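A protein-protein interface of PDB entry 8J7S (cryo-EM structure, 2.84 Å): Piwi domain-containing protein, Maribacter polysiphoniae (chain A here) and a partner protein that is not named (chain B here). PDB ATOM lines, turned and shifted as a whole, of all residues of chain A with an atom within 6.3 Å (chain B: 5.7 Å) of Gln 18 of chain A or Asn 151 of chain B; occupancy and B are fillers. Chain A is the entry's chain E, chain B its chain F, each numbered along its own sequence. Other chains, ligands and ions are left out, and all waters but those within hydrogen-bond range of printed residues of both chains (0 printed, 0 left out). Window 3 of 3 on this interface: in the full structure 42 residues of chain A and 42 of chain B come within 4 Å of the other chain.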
ATOM      1  N   ILE A  12      15.999 -19.177 -10.864  1.00  0.00           N
ATOM      2  CA  ILE A  12      16.457 -19.593  -9.544  1.00  0.00           C
ATOM      3  C   ILE A  12      17.975 -19.493  -9.518  1.00  0.00           C
ATOM      4  O   ILE A  12      18.652 -20.034 -10.398  1.00  0.00           O
ATOM      5  CB  ILE A  12      15.992 -21.018  -9.194  1.00  0.00           C
ATOM      6  CG1 ILE A  12      15.964 -21.904 -10.436  1.00  0.00           C
ATOM      7  CG2 ILE A  12      14.622 -20.976  -8.547  1.00  0.00           C
ATOM      8  CD1 ILE A  12      15.195 -23.193 -10.240  1.00  0.00           C
ATOM      9  N   LEU A  13      18.504 -18.802  -8.512  1.00  0.00           N
ATOM     10  CA  LEU A  13      19.926 -18.498  -8.445  1.00  0.00           C
ATOM     11  C   LEU A  13      20.686 -19.632  -7.769  1.00  0.00           C
ATOM     12  O   LEU A  13      20.348 -20.036  -6.653  1.00  0.00           O
ATOM     13  CB  LEU A  13      20.155 -17.186  -7.695  1.00  0.00           C
ATOM     14  CG  LEU A  13      21.534 -16.550  -7.859  1.00  0.00           C
ATOM     15  CD1 LEU A  13      21.734 -16.106  -9.292  1.00  0.00           C
ATOM     16  CD2 LEU A  13      21.702 -15.380  -6.912  1.00  0.00           C
ATOM     17  N   PHE A  14      21.705 -20.143  -8.453  1.00  0.00           N
ATOM     18  CA  PHE A  14      22.566 -21.205  -7.963  1.00  0.00           C
ATOM     19  C   PHE A  14      23.907 -20.632  -7.505  1.00  0.00           C
ATOM     20  O   PHE A  14      24.073 -19.417  -7.356  1.00  0.00           O
ATOM     21  CB  PHE A  14      22.731 -22.278  -9.036  1.00  0.00           C
ATOM     22  CG  PHE A  14      21.462 -23.008  -9.355  1.00  0.00           C
ATOM     23  CD1 PHE A  14      21.086 -24.117  -8.624  1.00  0.00           C
ATOM     24  CD2 PHE A  14      20.642 -22.581 -10.382  1.00  0.00           C
ATOM     25  CE1 PHE A  14      19.919 -24.787  -8.914  1.00  0.00           C
ATOM     26  CE2 PHE A  14      19.474 -23.249 -10.674  1.00  0.00           C
ATOM     27  CZ  PHE A  14      19.114 -24.352  -9.940  1.00  0.00           C
ATOM     28  N   ALA A  15      24.865 -21.521  -7.247  1.00  0.00           N
ATOM     29  CA  ALA A  15      26.154 -21.135  -6.689  1.00  0.00           C
ATOM     30  C   ALA A  15      26.863 -20.097  -7.556  1.00  0.00           C
ATOM     31  O   ALA A  15      26.705 -20.057  -8.778  1.00  0.00           O
ATOM     32  CB  ALA A  15      27.047 -22.364  -6.526  1.00  0.00           C
ATOM     33  N   HIS A  16      27.683 -19.277  -6.894  1.00  0.00           N
ATOM     34  CA  HIS A  16      28.390 -18.130  -7.480  1.00  0.00           C
ATOM     35  C   HIS A  16      27.518 -17.357  -8.467  1.00  0.00           C
ATOM     36  O   HIS A  16      27.943 -16.996  -9.568  1.00  0.00           O
ATOM     37  CB  HIS A  16      29.721 -18.541  -8.127  1.00  0.00           C
ATOM     38  CG  HIS A  16      29.785 -19.968  -8.574  1.00  0.00           C
ATOM     39  ND1 HIS A  16      29.011 -20.467  -9.600  1.00  0.00           N
ATOM     40  CD2 HIS A  16      30.543 -21.003  -8.139  1.00  0.00           C
ATOM     41  CE1 HIS A  16      29.283 -21.748  -9.772  1.00  0.00           C
ATOM     42  NE2 HIS A  16      30.210 -22.098  -8.898  1.00  0.00           N
ATOM     43  N   GLY A  17      26.285 -17.088  -8.051  1.00  0.00           N
ATOM     44  CA  GLY A  17      25.413 -16.185  -8.789  1.00  0.00           C
ATOM     45  C   GLY A  17      25.115 -16.594 -10.215  1.00  0.00           C
ATOM     46  O   GLY A  17      25.141 -15.748 -11.117  1.00  0.00           O
ATOM     47  N   GLN A  18      24.828 -17.871 -10.443  1.00  0.00           N
ATOM     48  CA  GLN A  18      24.554 -18.388 -11.779  1.00  0.00           C
ATOM     49  C   GLN A  18      23.055 -18.621 -11.914  1.00  0.00           C
ATOM     50  O   GLN A  18      22.513 -19.568 -11.334  1.00  0.00           O
ATOM     51  CB  GLN A  18      25.337 -19.672 -12.041  1.00  0.00           C
ATOM     52  CG  GLN A  18      26.745 -19.450 -12.564  1.00  0.00           C
ATOM     53  CD  GLN A  18      26.841 -18.298 -13.543  1.00  0.00           C
ATOM     54  OE1 GLN A  18      26.075 -18.215 -14.503  1.00  0.00           O
ATOM     55  NE2 GLN A  18      27.790 -17.401 -13.306  1.00  0.00           N
ATOM     56  N   LYS A  19      22.394 -17.762 -12.685  1.00  0.00           N
ATOM     57  CA  LYS A  19      20.963 -17.896 -12.906  1.00  0.00           C
ATOM     58  C   LYS A  19      20.664 -19.077 -13.819  1.00  0.00           C
ATOM     59  O   LYS A  19      21.445 -19.419 -14.709  1.00  0.00           O
ATOM     60  CB  LYS A  19      20.395 -16.616 -13.516  1.00  0.00           C
ATOM     61  CG  LYS A  19      20.539 -15.393 -12.637  1.00  0.00           C
ATOM     62  CD  LYS A  19      19.231 -14.636 -12.538  1.00  0.00           C
ATOM     63  CE  LYS A  19      18.982 -13.800 -13.777  1.00  0.00           C
ATOM     64  NZ  LYS A  19      18.486 -12.440 -13.431  1.00  0.00           N
ATOM     65  N   CYS A  20      19.514 -19.700 -13.589  1.00  0.00           N
ATOM     66  CA  CYS A  20      19.048 -20.806 -14.414  1.00  0.00           C
ATOM     67  C   CYS A  20      17.544 -20.924 -14.227  1.00  0.00           C
ATOM     68  O   CYS A  20      16.938 -20.191 -13.441  1.00  0.00           O
ATOM     69  CB  CYS A  20      19.767 -22.108 -14.055  1.00  0.00           C
ATOM     70  SG  CYS A  20      19.391 -23.489 -15.153  1.00  0.00           S
ATOM     71  N   LEU A  29      25.015 -28.404 -12.990  1.00  0.00           N
ATOM     72  CA  LEU A  29      25.980 -27.521 -13.632  1.00  0.00           C
ATOM     73  C   LEU A  29      26.838 -26.766 -12.623  1.00  0.00           C
ATOM     74  O   LEU A  29      28.059 -26.695 -12.777  1.00  0.00           O
ATOM     75  CB  LEU A  29      25.250 -26.531 -14.547  1.00  0.00           C
ATOM     76  CG  LEU A  29      25.109 -26.853 -16.041  1.00  0.00           C
ATOM     77  CD1 LEU A  29      26.423 -26.627 -16.773  1.00  0.00           C
ATOM     78  CD2 LEU A  29      24.592 -28.271 -16.271  1.00  0.00           C
ATOM     79  N   PHE A  30      26.222 -26.197 -11.588  1.00  0.00           N
ATOM     80  CA  PHE A  30      26.920 -25.329 -10.649  1.00  0.00           C
ATOM     81  C   PHE A  30      27.030 -25.919  -9.251  1.00  0.00           C
ATOM     82  O   PHE A  30      28.131 -26.000  -8.702  1.00  0.00           O
ATOM     83  CB  PHE A  30      26.212 -23.969 -10.582  1.00  0.00           C
ATOM     84  CG  PHE A  30      25.849 -23.414 -11.927  1.00  0.00           C
ATOM     85  CD1 PHE A  30      26.831 -23.092 -12.847  1.00  0.00           C
ATOM     86  CD2 PHE A  30      24.524 -23.227 -12.277  1.00  0.00           C
ATOM     87  CE1 PHE A  30      26.499 -22.588 -14.087  1.00  0.00           C
ATOM     88  CE2 PHE A  30      24.186 -22.723 -13.515  1.00  0.00           C
ATOM     89  CZ  PHE A  30      25.175 -22.402 -14.420  1.00  0.00           C
ATOM     90  N   ASP B 146      35.455 -19.378 -14.459  1.00  0.00           N
ATOM     91  CA  ASP B 146      34.226 -18.595 -14.371  1.00  0.00           C
ATOM     92  C   ASP B 146      33.083 -19.446 -14.899  1.00  0.00           C
ATOM     93  O   ASP B 146      33.142 -19.923 -16.036  1.00  0.00           O
ATOM     94  CB  ASP B 146      34.346 -17.291 -15.159  1.00  0.00           C
ATOM     95  CG  ASP B 146      33.414 -16.213 -14.644  1.00  0.00           C
ATOM     96  OD1 ASP B 146      32.775 -16.430 -13.594  1.00  0.00           O
ATOM     97  OD2 ASP B 146      33.322 -15.147 -15.288  1.00  0.00           O
ATOM     98  N   ALA B 147      32.049 -19.637 -14.077  1.00  0.00           N
ATOM     99  CA  ALA B 147      30.913 -20.456 -14.479  1.00  0.00           C
ATOM    100  C   ALA B 147      30.049 -19.775 -15.530  1.00  0.00           C
ATOM    101  O   ALA B 147      29.222 -20.443 -16.161  1.00  0.00           O
ATOM    102  CB  ALA B 147      30.066 -20.813 -13.257  1.00  0.00           C
ATOM    103  N   SER B 148      30.218 -18.465 -15.727  1.00  0.00           N
ATOM    104  CA  SER B 148      29.422 -17.755 -16.722  1.00  0.00           C
ATOM    105  C   SER B 148      29.685 -18.275 -18.129  1.00  0.00           C
ATOM    106  O   SER B 148      28.768 -18.310 -18.953  1.00  0.00           O
ATOM    107  CB  SER B 148      29.708 -16.257 -16.646  1.00  0.00           C
ATOM    108  OG  SER B 148      31.039 -15.971 -17.039  1.00  0.00           O
ATOM    109  N   LYS B 149      30.921 -18.685 -18.422  1.00  0.00           N
ATOM    110  CA  LYS B 149      31.227 -19.238 -19.738  1.00  0.00           C
ATOM    111  C   LYS B 149      30.458 -20.531 -19.980  1.00  0.00           C
ATOM    112  O   LYS B 149      29.872 -20.731 -21.051  1.00  0.00           O
ATOM    113  CB  LYS B 149      32.731 -19.479 -19.867  1.00  0.00           C
ATOM    114  CG  LYS B 149      33.576 -18.223 -19.781  1.00  0.00           C
ATOM    115  CD  LYS B 149      35.054 -18.568 -19.705  1.00  0.00           C
ATOM    116  CE  LYS B 149      35.458 -18.952 -18.291  1.00  0.00           C
ATOM    117  NZ  LYS B 149      36.745 -19.700 -18.258  1.00  0.00           N
ATOM    118  N   SER B 150      30.448 -21.422 -18.987  1.00  0.00           N
ATOM    119  CA  SER B 150      29.701 -22.667 -19.120  1.00  0.00           C
ATOM    120  C   SER B 150      28.204 -22.405 -19.215  1.00  0.00           C
ATOM    121  O   SER B 150      27.502 -23.074 -19.978  1.00  0.00           O
ATOM    122  CB  SER B 150      30.010 -23.596 -17.949  1.00  0.00           C
ATOM    123  OG  SER B 150      29.347 -24.838 -18.099  1.00  0.00           O
ATOM    124  N   ASN B 151      27.699 -21.443 -18.440  1.00  0.00           N
ATOM    125  CA  ASN B 151      26.283 -21.099 -18.520  1.00  0.00           C
ATOM    126  C   ASN B 151      25.920 -20.583 -19.906  1.00  0.00           C
ATOM    127  O   ASN B 151      24.892 -20.971 -20.474  1.00  0.00           O
ATOM    128  CB  ASN B 151      25.939 -20.058 -17.457  1.00  0.00           C
ATOM    129  CG  ASN B 151      24.462 -20.021 -17.132  1.00  0.00           C
ATOM    130  OD1 ASN B 151      23.672 -20.787 -17.683  1.00  0.00           O
ATOM    131  ND2 ASN B 151      24.080 -19.122 -16.234  1.00  0.00           N
ATOM    132  N   LEU B 152      26.755 -19.703 -20.465  1.00  0.00           N
ATOM    133  CA  LEU B 152      26.505 -19.175 -21.800  1.00  0.00           C
ATOM    134  C   LEU B 152      26.538 -20.283 -22.843  1.00  0.00           C
ATOM    135  O   LEU B 152      25.684 -20.331 -23.735  1.00  0.00           O
ATOM    136  CB  LEU B 152      27.534 -18.097 -22.133  1.00  0.00           C
ATOM    137  CG  LEU B 152      26.994 -16.749 -22.605  1.00  0.00           C
ATOM    138  CD1 LEU B 152      28.137 -15.847 -23.040  1.00  0.00           C
ATOM    139  CD2 LEU B 152      25.989 -16.933 -23.728  1.00  0.00           C
ATOM    140  N   LEU B 153      27.520 -21.180 -22.747  1.00  0.00           N
ATOM    141  CA  LEU B 153      27.599 -22.304 -23.675  1.00  0.00           C
ATOM    142  C   LEU B 153      26.366 -23.196 -23.574  1.00  0.00           C
ATOM    143  O   LEU B 153      25.808 -23.624 -24.595  1.00  0.00           O
ATOM    144  CB  LEU B 153      28.878 -23.093 -23.397  1.00  0.00           C
ATOM    145  CG  LEU B 153      29.513 -23.923 -24.507  1.00  0.00           C
ATOM    146  CD1 LEU B 153      31.020 -23.825 -24.423  1.00  0.00           C
ATOM    147  CD2 LEU B 153      29.080 -25.366 -24.348  1.00  0.00           C
ATOM    148  N   TYR B 154      25.919 -23.474 -22.348  1.00  0.00           N
ATOM    149  CA  TYR B 154      24.734 -24.296 -22.143  1.00  0.00           C
ATOM    150  C   TYR B 154      23.498 -23.639 -22.740  1.00  0.00           C
ATOM    151  O   TYR B 154      22.672 -24.309 -23.371  1.00  0.00           O
ATOM    152  CB  TYR B 154      24.542 -24.553 -20.647  1.00  0.00           C
ATOM    153  CG  TYR B 154      23.295 -25.331 -20.303  1.00  0.00           C
ATOM    154  CD1 TYR B 154      23.185 -26.675 -20.619  1.00  0.00           C
ATOM    155  CD2 TYR B 154      22.225 -24.717 -19.666  1.00  0.00           C
ATOM    156  CE1 TYR B 154      22.049 -27.388 -20.311  1.00  0.00           C
ATOM    157  CE2 TYR B 154      21.083 -25.423 -19.355  1.00  0.00           C
ATOM    158  CZ  TYR B 154      21.001 -26.759 -19.680  1.00  0.00           C
ATOM    159  OH  TYR B 154      19.867 -27.474 -19.372  1.00  0.00           O
ATOM    160  N   GLN B 155      23.350 -22.327 -22.544  1.00  0.00           N
ATOM    161  CA  GLN B 155      22.209 -21.619 -23.115  1.00  0.00           C
ATOM    162  C   GLN B 155      22.261 -21.623 -24.638  1.00  0.00           C
ATOM    163  O   GLN B 155      21.233 -21.802 -25.301  1.00  0.00           O
ATOM    164  CB  GLN B 155      22.160 -20.188 -22.587  1.00  0.00           C
ATOM    165  CG  GLN B 155      21.183 -19.980 -21.447  1.00  0.00           C
ATOM    166  CD  GLN B 155      21.727 -19.051 -20.382  1.00  0.00           C
ATOM    167  OE1 GLN B 155      22.724 -18.361 -20.595  1.00  0.00           O
ATOM    168  NE2 GLN B 155      21.075 -19.027 -19.226  1.00  0.00           N
ATOM    169  N   GLN B 156      23.449 -21.422 -25.210  1.00  0.00           N
ATOM    170  CA  GLN B 156      23.570 -21.348 -26.662  1.00  0.00           C
ATOM    171  C   GLN B 156      23.264 -22.686 -27.318  1.00  0.00           C
ATOM    172  O   GLN B 156      22.458 -22.760 -28.253  1.00  0.00           O
ATOM    173  CB  GLN B 156      24.971 -20.879 -27.052  1.00  0.00           C
ATOM    174  CG  GLN B 156      25.269 -19.428 -26.735  1.00  0.00           C
ATOM    175  CD  GLN B 156      26.747 -19.110 -26.838  1.00  0.00           C
ATOM    176  OE1 GLN B 156      27.573 -20.002 -27.019  1.00  0.00           O
ATOM    177  NE2 GLN B 156      27.086 -17.832 -26.726  1.00  0.00           N
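The backbone carbonyl oxygen (O) of Lys 19 of chain A sits at hydrogen-bond distance from the side-chain amide nitrogen (ND2) of Asn 151 of chain B (3.1 Å). The side-chain amide oxygen (OE1) of Gln 18 of chain A is in hydrogen-bond range of the side-chain amide nitrogen (ND2) of Asn 151 of chain B, at 2.8 Å.
O of Asn 151 of chain B lies close to OE1 of Gln 155 of chain B, at 3.4 Å. The side-chain hydroxyl (OG) of Ser 148 of chain B lies within hydrogen-bond range of the side-chain carboxylate (OD2) of Asp 146 of chain B (3.0 Å).
Among the printed residues, pairs that only touch across the chains: His 16 of chain A with Ala 147 of chain B (3.7 Å), Gln 18 of chain A with Ala 147 of chain B (3.7 Å), Gln 18 of chain A with Ser 148 of chain B (3.6 Å), Leu 29 of chain A with Ser 150 of chain B (3.7 Å), Phe 30 of chain A with Ala 147 of chain B (3.98 Å) and Phe 30 of chain A with Asn 151 of chain B (3.7 Å).
Gln 18 of chain A touches three residues of chain B. Asn 151 of chain B touches just these residues of chain A: Gln 18 (2.8 Å), Lys 19 (3.1 Å) and Phe 30 (3.7 Å). Printed residues of chain B within 4 Å of Leu 29 of chain A: Ser 150 (3.7 Å). Printed residues of chain A within 4 Å of Ser 150 of chain B: Leu 29 (3.7 Å). Printed residues of chain A within 4 Å of Ala 147 of chain B: His 16, Gln 18 and Phe 30. Of the printed residues of chain B, Lys 19 of chain A touches Asn 151. Of the printed residues of chain B, Phe 30 of chain A touches Ala 147 and Asn 151. Leu 153 of chain B touches none of the printed residues of chain A. Gln 156 of chain B touches none of the printed residues of chain A. The nearest residue of chain B that does not touch Gln 18 of chain A is Asp 146 of chain B (5.1 Å). The nearest residue of chain A that does not touch Asn 151 of chain B is Cys 20 of chain A (5.3 Å). The nearest printed residue of chain A that does not touch Ser 150 of chain B is Phe 30 of chain A (5.3 Å).
Hydrophobic or aromatic side chains of chain A that line the printed part of chain B: His 16, Leu 29 and Phe 30. Along chain B the printed residues that touch a printed residue of chain A span positions 147 to 151.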
